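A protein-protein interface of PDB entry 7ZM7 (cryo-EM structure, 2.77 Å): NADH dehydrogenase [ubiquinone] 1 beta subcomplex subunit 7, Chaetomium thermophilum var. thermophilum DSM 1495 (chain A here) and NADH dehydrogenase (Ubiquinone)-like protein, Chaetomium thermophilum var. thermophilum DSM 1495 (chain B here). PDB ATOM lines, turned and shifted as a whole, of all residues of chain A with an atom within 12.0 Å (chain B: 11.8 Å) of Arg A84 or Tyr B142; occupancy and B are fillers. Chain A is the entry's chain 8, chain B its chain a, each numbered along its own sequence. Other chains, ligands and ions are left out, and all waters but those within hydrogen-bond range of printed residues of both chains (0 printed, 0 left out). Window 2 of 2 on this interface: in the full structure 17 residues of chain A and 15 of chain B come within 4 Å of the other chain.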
ATOM      1  N   MET A  73       3.786  -3.839  16.065  1.00  0.00           N
ATOM      2  CA  MET A  73       4.277  -2.863  17.031  1.00  0.00           C
ATOM      3  C   MET A  73       5.388  -3.451  17.889  1.00  0.00           C
ATOM      4  O   MET A  73       6.379  -2.773  18.183  1.00  0.00           O
ATOM      5  CB  MET A  73       3.135  -2.369  17.912  1.00  0.00           C
ATOM      6  CG  MET A  73       3.526  -1.239  18.846  1.00  0.00           C
ATOM      7  SD  MET A  73       3.960   0.276  17.981  1.00  0.00           S
ATOM      8  CE  MET A  73       4.998   1.069  19.205  1.00  0.00           C
ATOM      9  N   GLU A  74       5.236  -4.709  18.315  1.00  0.00           N
ATOM     10  CA  GLU A  74       6.283  -5.346  19.108  1.00  0.00           C
ATOM     11  C   GLU A  74       7.586  -5.416  18.327  1.00  0.00           C
ATOM     12  O   GLU A  74       8.671  -5.266  18.899  1.00  0.00           O
ATOM     13  CB  GLU A  74       5.852  -6.746  19.544  1.00  0.00           C
ATOM     14  CG  GLU A  74       4.704  -6.774  20.535  1.00  0.00           C
ATOM     15  CD  GLU A  74       3.938  -8.078  20.488  1.00  0.00           C
ATOM     16  OE1 GLU A  74       4.155  -8.858  19.538  1.00  0.00           O
ATOM     17  OE2 GLU A  74       3.126  -8.326  21.403  1.00  0.00           O
ATOM     18  N   LEU A  76       8.436  -3.155  16.163  1.00  0.00           N
ATOM     19  CA  LEU A  76       8.940  -1.789  16.248  1.00  0.00           C
ATOM     20  C   LEU A  76       9.588  -1.523  17.601  1.00  0.00           C
ATOM     21  O   LEU A  76      10.615  -0.839  17.676  1.00  0.00           O
ATOM     22  CB  LEU A  76       7.811  -0.794  15.991  1.00  0.00           C
ATOM     23  CG  LEU A  76       8.241   0.670  15.993  1.00  0.00           C
ATOM     24  CD1 LEU A  76       9.231   0.919  14.872  1.00  0.00           C
ATOM     25  CD2 LEU A  76       7.041   1.588  15.864  1.00  0.00           C
ATOM     26  N   ARG A  77       9.003  -2.047  18.680  1.00  0.00           N
ATOM     27  CA  ARG A  77       9.563  -1.810  20.007  1.00  0.00           C
ATOM     28  C   ARG A  77      10.961  -2.400  20.136  1.00  0.00           C
ATOM     29  O   ARG A  77      11.867  -1.753  20.675  1.00  0.00           O
ATOM     30  CB  ARG A  77       8.644  -2.386  21.083  1.00  0.00           C
ATOM     31  CG  ARG A  77       9.165  -2.176  22.497  1.00  0.00           C
ATOM     32  CD  ARG A  77       8.178  -2.669  23.536  1.00  0.00           C
ATOM     33  NE  ARG A  77       6.961  -1.866  23.548  1.00  0.00           N
ATOM     34  CZ  ARG A  77       5.781  -2.297  23.121  1.00  0.00           C
ATOM     35  NH1 ARG A  77       4.725  -1.499  23.168  1.00  0.00           N
ATOM     36  NH2 ARG A  77       5.658  -3.529  22.644  1.00  0.00           N
ATOM     37  N   GLU A  78      11.159  -3.626  19.648  1.00  0.00           N
ATOM     38  CA  GLU A  78      12.474  -4.246  19.744  1.00  0.00           C
ATOM     39  C   GLU A  78      13.477  -3.617  18.788  1.00  0.00           C
ATOM     40  O   GLU A  78      14.686  -3.765  18.992  1.00  0.00           O
ATOM     41  CB  GLU A  78      12.375  -5.751  19.490  1.00  0.00           C
ATOM     42  CG  GLU A  78      11.849  -6.122  18.118  1.00  0.00           C
ATOM     43  CD  GLU A  78      12.952  -6.274  17.089  1.00  0.00           C
ATOM     44  OE1 GLU A  78      14.113  -6.493  17.492  1.00  0.00           O
ATOM     45  OE2 GLU A  78      12.659  -6.169  15.881  1.00  0.00           O
ATOM     46  N   ALA A  79      13.004  -2.922  17.753  1.00  0.00           N
ATOM     47  CA  ALA A  79      13.918  -2.209  16.870  1.00  0.00           C
ATOM     48  C   ALA A  79      14.565  -1.025  17.574  1.00  0.00           C
ATOM     49  O   ALA A  79      15.670  -0.613  17.204  1.00  0.00           O
ATOM     50  CB  ALA A  79      13.183  -1.744  15.615  1.00  0.00           C
ATOM     51  N   LYS A  80      13.897  -0.465  18.580  1.00  0.00           N
ATOM     52  CA  LYS A  80      14.418   0.654  19.350  1.00  0.00           C
ATOM     53  C   LYS A  80      14.964   0.230  20.705  1.00  0.00           C
ATOM     54  O   LYS A  80      15.217   1.087  21.557  1.00  0.00           O
ATOM     55  CB  LYS A  80      13.334   1.716  19.536  1.00  0.00           C
ATOM     56  CG  LYS A  80      12.854   2.325  18.238  1.00  0.00           C
ATOM     57  CD  LYS A  80      13.974   3.080  17.554  1.00  0.00           C
ATOM     58  CE  LYS A  80      14.318   4.350  18.309  1.00  0.00           C
ATOM     59  NZ  LYS A  80      15.365   5.142  17.608  1.00  0.00           N
ATOM     60  N   GLY A  81      15.144  -1.067  20.926  1.00  0.00           N
ATOM     61  CA  GLY A  81      15.635  -1.548  22.204  1.00  0.00           C
ATOM     62  C   GLY A  81      14.681  -1.323  23.356  1.00  0.00           C
ATOM     63  O   GLY A  81      15.124  -1.073  24.483  1.00  0.00           O
ATOM     64  N   GLY A  82      13.379  -1.410  23.100  1.00  0.00           N
ATOM     65  CA  GLY A  82      12.397  -1.262  24.162  1.00  0.00           C
ATOM     66  C   GLY A  82      12.393   0.097  24.829  1.00  0.00           C
ATOM     67  O   GLY A  82      12.255   0.183  26.056  1.00  0.00           O
ATOM     68  N   ALA A  83      12.539   1.162  24.052  1.00  0.00           N
ATOM     69  CA  ALA A  83      12.493   2.510  24.592  1.00  0.00           C
ATOM     70  C   ALA A  83      11.068   3.056  24.540  1.00  0.00           C
ATOM     71  O   ALA A  83      10.159   2.449  23.972  1.00  0.00           O
ATOM     72  CB  ALA A  83      13.448   3.426  23.829  1.00  0.00           C
ATOM     73  N   ARG A  84      10.880   4.222  25.152  1.00  0.00           N
ATOM     74  CA  ARG A  84       9.568   4.856  25.174  1.00  0.00           C
ATOM     75  C   ARG A  84       9.227   5.374  23.785  1.00  0.00           C
ATOM     76  O   ARG A  84      10.048   6.035  23.143  1.00  0.00           O
ATOM     77  CB  ARG A  84       9.546   5.991  26.196  1.00  0.00           C
ATOM     78  CG  ARG A  84       8.151   6.403  26.606  1.00  0.00           C
ATOM     79  CD  ARG A  84       7.431   5.216  27.207  1.00  0.00           C
ATOM     80  NE  ARG A  84       8.211   4.598  28.272  1.00  0.00           N
ATOM     81  CZ  ARG A  84       8.049   4.870  29.560  1.00  0.00           C
ATOM     82  NH1 ARG A  84       7.112   5.723  29.944  1.00  0.00           N
ATOM     83  NH2 ARG A  84       8.805   4.267  30.467  1.00  0.00           N
ATOM     84  N   SER A  85       8.020   5.070  23.314  1.00  0.00           N
ATOM     85  CA  SER A  85       7.596   5.471  21.983  1.00  0.00           C
ATOM     86  C   SER A  85       6.255   6.187  21.954  1.00  0.00           C
ATOM     87  O   SER A  85       5.800   6.566  20.869  1.00  0.00           O
ATOM     88  CB  SER A  85       7.535   4.251  21.056  1.00  0.00           C
ATOM     89  OG  SER A  85       7.051   4.615  19.777  1.00  0.00           O
ATOM     90  N   ASN A  86       5.609   6.385  23.098  1.00  0.00           N
ATOM     91  CA  ASN A  86       4.296   7.022  23.125  1.00  0.00           C
ATOM     92  C   ASN A  86       4.383   8.482  23.558  1.00  0.00           C
ATOM     93  O   ASN A  86       5.382   8.909  24.133  1.00  0.00           O
ATOM     94  CB  ASN A  86       3.353   6.256  24.051  1.00  0.00           C
ATOM     95  CG  ASN A  86       3.885   6.143  25.462  1.00  0.00           C
ATOM     96  OD1 ASN A  86       4.983   6.602  25.761  1.00  0.00           O
ATOM     97  ND2 ASN A  86       3.111   5.516  26.337  1.00  0.00           N
ATOM     98  N   LEU B 134       2.879  12.093  43.636  1.00  0.00           N
ATOM     99  CA  LEU B 134       2.138  11.028  42.973  1.00  0.00           C
ATOM    100  C   LEU B 134       2.276  11.128  41.463  1.00  0.00           C
ATOM    101  O   LEU B 134       2.359  10.110  40.768  1.00  0.00           O
ATOM    102  CB  LEU B 134       0.669  11.079  43.378  1.00  0.00           C
ATOM    103  CG  LEU B 134      -0.181   9.904  42.903  1.00  0.00           C
ATOM    104  CD1 LEU B 134       0.313   8.607  43.518  1.00  0.00           C
ATOM    105  CD2 LEU B 134      -1.635  10.140  43.247  1.00  0.00           C
ATOM    106  N   CYS B 135       2.288  12.350  40.933  1.00  0.00           N
ATOM    107  CA  CYS B 135       2.481  12.525  39.499  1.00  0.00           C
ATOM    108  C   CYS B 135       3.867  12.062  39.072  1.00  0.00           C
ATOM    109  O   CYS B 135       4.029  11.460  38.005  1.00  0.00           O
ATOM    110  CB  CYS B 135       2.260  13.989  39.122  1.00  0.00           C
ATOM    111  SG  CYS B 135       2.339  14.332  37.356  1.00  0.00           S
ATOM    112  N   TYR B 136       4.881  12.331  39.898  1.00  0.00           N
ATOM    113  CA  TYR B 136       6.253  12.020  39.515  1.00  0.00           C
ATOM    114  C   TYR B 136       6.468  10.521  39.359  1.00  0.00           C
ATOM    115  O   TYR B 136       7.138  10.083  38.417  1.00  0.00           O
ATOM    116  CB  TYR B 136       7.226  12.596  40.541  1.00  0.00           C
ATOM    117  CG  TYR B 136       8.672  12.248  40.278  1.00  0.00           C
ATOM    118  CD1 TYR B 136       9.418  12.958  39.349  1.00  0.00           C
ATOM    119  CD2 TYR B 136       9.294  11.218  40.968  1.00  0.00           C
ATOM    120  CE1 TYR B 136      10.740  12.646  39.108  1.00  0.00           C
ATOM    121  CE2 TYR B 136      10.615  10.899  40.734  1.00  0.00           C
ATOM    122  CZ  TYR B 136      11.333  11.617  39.804  1.00  0.00           C
ATOM    123  OH  TYR B 136      12.650  11.301  39.567  1.00  0.00           O
ATOM    124  N   VAL B 137       5.915   9.719  40.269  1.00  0.00           N
ATOM    125  CA  VAL B 137       6.154   8.283  40.204  1.00  0.00           C
ATOM    126  C   VAL B 137       5.500   7.680  38.969  1.00  0.00           C
ATOM    127  O   VAL B 137       6.006   6.704  38.403  1.00  0.00           O
ATOM    128  CB  VAL B 137       5.681   7.600  41.502  1.00  0.00           C
ATOM    129  CG1 VAL B 137       4.194   7.793  41.707  1.00  0.00           C
ATOM    130  CG2 VAL B 137       6.037   6.124  41.494  1.00  0.00           C
ATOM    131  N   VAL B 138       4.379   8.246  38.520  1.00  0.00           N
ATOM    132  CA  VAL B 138       3.707   7.719  37.337  1.00  0.00           C
ATOM    133  C   VAL B 138       4.556   7.944  36.093  1.00  0.00           C
ATOM    134  O   VAL B 138       4.619   7.086  35.205  1.00  0.00           O
ATOM    135  CB  VAL B 138       2.310   8.348  37.195  1.00  0.00           C
ATOM    136  CG1 VAL B 138       1.644   7.884  35.913  1.00  0.00           C
ATOM    137  CG2 VAL B 138       1.456   8.000  38.393  1.00  0.00           C
ATOM    138  N   LYS B 139       5.221   9.098  36.005  1.00  0.00           N
ATOM    139  CA  LYS B 139       6.038   9.389  34.832  1.00  0.00           C
ATOM    140  C   LYS B 139       7.197   8.412  34.711  1.00  0.00           C
ATOM    141  O   LYS B 139       7.567   8.008  33.603  1.00  0.00           O
ATOM    142  CB  LYS B 139       6.558  10.824  34.890  1.00  0.00           C
ATOM    143  CG  LYS B 139       7.179  11.310  33.590  1.00  0.00           C
ATOM    144  CD  LYS B 139       8.695  11.211  33.618  1.00  0.00           C
ATOM    145  CE  LYS B 139       9.295  12.167  34.634  1.00  0.00           C
ATOM    146  NZ  LYS B 139      10.782  12.084  34.658  1.00  0.00           N
ATOM    147  N   LEU B 140       7.793   8.032  35.841  1.00  0.00           N
ATOM    148  CA  LEU B 140       8.929   7.120  35.806  1.00  0.00           C
ATOM    149  C   LEU B 140       8.533   5.756  35.258  1.00  0.00           C
ATOM    150  O   LEU B 140       9.293   5.145  34.501  1.00  0.00           O
ATOM    151  CB  LEU B 140       9.535   6.983  37.200  1.00  0.00           C
ATOM    152  CG  LEU B 140      10.744   7.874  37.484  1.00  0.00           C
ATOM    153  CD1 LEU B 140      10.351   9.338  37.449  1.00  0.00           C
ATOM    154  CD2 LEU B 140      11.360   7.518  38.825  1.00  0.00           C
ATOM    155  N   THR B 141       7.354   5.258  35.629  1.00  0.00           N
ATOM    156  CA  THR B 141       6.922   3.913  35.248  1.00  0.00           C
ATOM    157  C   THR B 141       5.489   3.963  34.729  1.00  0.00           C
ATOM    158  O   THR B 141       4.543   3.733  35.485  1.00  0.00           O
ATOM    159  CB  THR B 141       7.049   2.961  36.429  1.00  0.00           C
ATOM    160  OG1 THR B 141       8.358   3.079  36.997  1.00  0.00           O
ATOM    161  CG2 THR B 141       6.830   1.528  35.978  1.00  0.00           C
ATOM    162  N   TYR B 142       5.329   4.251  33.441  1.00  0.00           N
ATOM    163  CA  TYR B 142       4.024   4.182  32.808  1.00  0.00           C
ATOM    164  C   TYR B 142       4.178   3.530  31.443  1.00  0.00           C
ATOM    165  O   TYR B 142       5.217   3.688  30.791  1.00  0.00           O
ATOM    166  CB  TYR B 142       3.366   5.569  32.684  1.00  0.00           C
ATOM    167  CG  TYR B 142       3.793   6.416  31.515  1.00  0.00           C
ATOM    168  CD1 TYR B 142       3.128   6.338  30.305  1.00  0.00           C
ATOM    169  CD2 TYR B 142       4.834   7.325  31.630  1.00  0.00           C
ATOM    170  CE1 TYR B 142       3.504   7.116  29.236  1.00  0.00           C
ATOM    171  CE2 TYR B 142       5.213   8.113  30.566  1.00  0.00           C
ATOM    172  CZ  TYR B 142       4.544   8.001  29.372  1.00  0.00           C
ATOM    173  OH  TYR B 142       4.914   8.773  28.303  1.00  0.00           O
ATOM    174  N   PRO B 143       3.167   2.802  30.986  1.00  0.00           N
ATOM    175  CA  PRO B 143       3.371   1.878  29.869  1.00  0.00           C
ATOM    176  C   PRO B 143       3.627   2.582  28.551  1.00  0.00           C
ATOM    177  O   PRO B 143       3.227   3.728  28.333  1.00  0.00           O
ATOM    178  CB  PRO B 143       2.056   1.097  29.819  1.00  0.00           C
ATOM    179  CG  PRO B 143       1.064   2.034  30.377  1.00  0.00           C
ATOM    180  CD  PRO B 143       1.778   2.767  31.469  1.00  0.00           C
ATOM    181  N   ASP B 144       4.316   1.872  27.665  1.00  0.00           N
ATOM    182  CA  ASP B 144       4.373   2.273  26.270  1.00  0.00           C
ATOM    183  C   ASP B 144       3.078   1.884  25.573  1.00  0.00           C
ATOM    184  O   ASP B 144       2.355   0.986  26.012  1.00  0.00           O
ATOM    185  CB  ASP B 144       5.567   1.622  25.577  1.00  0.00           C
ATOM    186  CG  ASP B 144       5.759   2.114  24.159  1.00  0.00           C
ATOM    187  OD1 ASP B 144       6.224   3.259  23.982  1.00  0.00           O
ATOM    188  OD2 ASP B 144       5.447   1.353  23.219  1.00  0.00           O
ATOM    189  N   ARG B 145       2.775   2.578  24.485  1.00  0.00           N
ATOM    190  CA  ARG B 145       1.574   2.270  23.727  1.00  0.00           C
ATOM    191  C   ARG B 145       1.707   0.908  23.060  1.00  0.00           C
ATOM    192  O   ARG B 145       2.802   0.482  22.686  1.00  0.00           O
ATOM    193  CB  ARG B 145       1.314   3.362  22.692  1.00  0.00           C
ATOM    194  CG  ARG B 145       2.296   3.398  21.556  1.00  0.00           C
ATOM    195  CD  ARG B 145       1.988   4.561  20.651  1.00  0.00           C
ATOM    196  NE  ARG B 145       0.620   4.507  20.153  1.00  0.00           N
ATOM    197  CZ  ARG B 145      -0.060   5.567  19.736  1.00  0.00           C
ATOM    198  NH1 ARG B 145      -1.301   5.430  19.295  1.00  0.00           N
ATOM    199  NH2 ARG B 145       0.500   6.767  19.769  1.00  0.00           N
ATOM    200  N   VAL B 146       0.579   0.216  22.925  1.00  0.00           N
ATOM    201  CA  VAL B 146       0.557  -1.149  22.417  1.00  0.00           C
ATOM    202  C   VAL B 146      -0.086  -1.244  21.046  1.00  0.00           C
ATOM    203  O   VAL B 146       0.109  -2.246  20.346  1.00  0.00           O
ATOM    204  CB  VAL B 146      -0.150  -2.088  23.414  1.00  0.00           C
ATOM    205  CG1 VAL B 146      -1.611  -1.713  23.541  1.00  0.00           C
ATOM    206  CG2 VAL B 146       0.021  -3.549  23.030  1.00  0.00           C
ATOM    207  N   SER B 147      -0.814  -0.219  20.624  1.00  0.00           N
ATOM    208  CA  SER B 147      -1.543  -0.234  19.367  1.00  0.00           C
ATOM    209  C   SER B 147      -0.948   0.782  18.406  1.00  0.00           C
ATOM    210  O   SER B 147      -0.766   1.952  18.756  1.00  0.00           O
ATOM    211  CB  SER B 147      -3.020   0.076  19.591  1.00  0.00           C
ATOM    212  OG  SER B 147      -3.787  -0.200  18.433  1.00  0.00           O
ATOM    213  N   ASP B 174       6.578   7.392  13.110  1.00  0.00           N
ATOM    214  CA  ASP B 174       6.050   7.187  14.452  1.00  0.00           C
ATOM    215  C   ASP B 174       7.122   7.447  15.502  1.00  0.00           C
ATOM    216  O   ASP B 174       6.817   7.804  16.638  1.00  0.00           O
ATOM    217  CB  ASP B 174       5.500   5.772  14.612  1.00  0.00           C
ATOM    218  CG  ASP B 174       4.931   5.524  15.996  1.00  0.00           C
ATOM    219  OD1 ASP B 174       4.283   6.439  16.544  1.00  0.00           O
ATOM    220  OD2 ASP B 174       5.134   4.420  16.539  1.00  0.00           O
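The guanidinium group (NH1) of Arg A84 sits at hydrogen-bond distance from the backbone carbonyl oxygen (O) of Tyr B142 (2.9 Å).
OD1 of Asp B144 sits at hydrogen-bond distance from N of Asn A86.
The guanidinium group (NH1) of Arg A77 lies within salt-bridge range of the side-chain carboxylate (OD2) of Asp B144, at 2.9 Å.
The backbone carbonyl oxygen (O) of Arg B145 is in hydrogen-bond range of the guanidinium group (NH1) of Arg A77.
The side-chain carboxylate (OD1) of Asp B144 lies within hydrogen-bond range of the backbone NH (N) of Ser A85 (2.6 Å).
The side-chain amide nitrogen of Asn A86 sits close to the backbone NH of Arg B145 (3.5 Å).
ND2 of Asn A86 is in hydrogen-bond range of O of Pro B143, at 2.7 Å.
The side-chain hydroxyl (OH) of Tyr B142 lies within hydrogen-bond range of the side-chain amide oxygen (OD1) of Asn A86, at 3.3 Å.
The guanidinium group (NE) of Arg B145 lies within hydrogen-bond range of the backbone carbonyl oxygen (O) of Ser B147, at 3.2 Å.
The backbone NH (N) of Gly A82 lies within hydrogen-bond range of the backbone carbonyl oxygen (O) of Arg A77.
Val B146 touches Met A73.
Leu A76 touches Asp B174.
Asp B144 touches Arg A84.
Asp B174 touches Ser A85 (OD2 to OG, 3.8 Å).
Arg A84 touches just these residues of chain B: Tyr B142 and Asp B144.
Tyr B142 touches two residues of chain A.
Printed residues of chain B within 4 Å of Ser A85: Asp B144 and Asp B174.
Of chain B, only Tyr B142 (3.3 Å), Pro B143 (2.7 Å), Asp B144 (3.3 Å) and Arg B145 (3.5 Å) come within 4 Å of Asn A86.
No residue of chain A comes within 4 Å of Val B138.
Of chain A, only Asn A86 (2.7 Å) comes within 4 Å of Pro B143.
Printed residues of chain A within 4 Å of Arg B145: Arg A77 and Asn A86.
Printed residues of chain A within 4 Å of Asp B144: Arg A77, Arg A84, Ser A85 and Asn A86.
Leu B134 touches none of the printed residues of chain A.
Ser B147 touches none of the printed residues of chain A.
Of the 13 printed residues of chain A, 6 touch a printed residue of chain B.
Hydrophobic or aromatic side chains of chain A within 4 Å of the printed part of chain B: Met A73 and Leu A76.
Along chain A the printed residues that touch a printed residue of chain B span positions 73 to 86.
Among the printed residues, 12 pairs touch across the chains.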
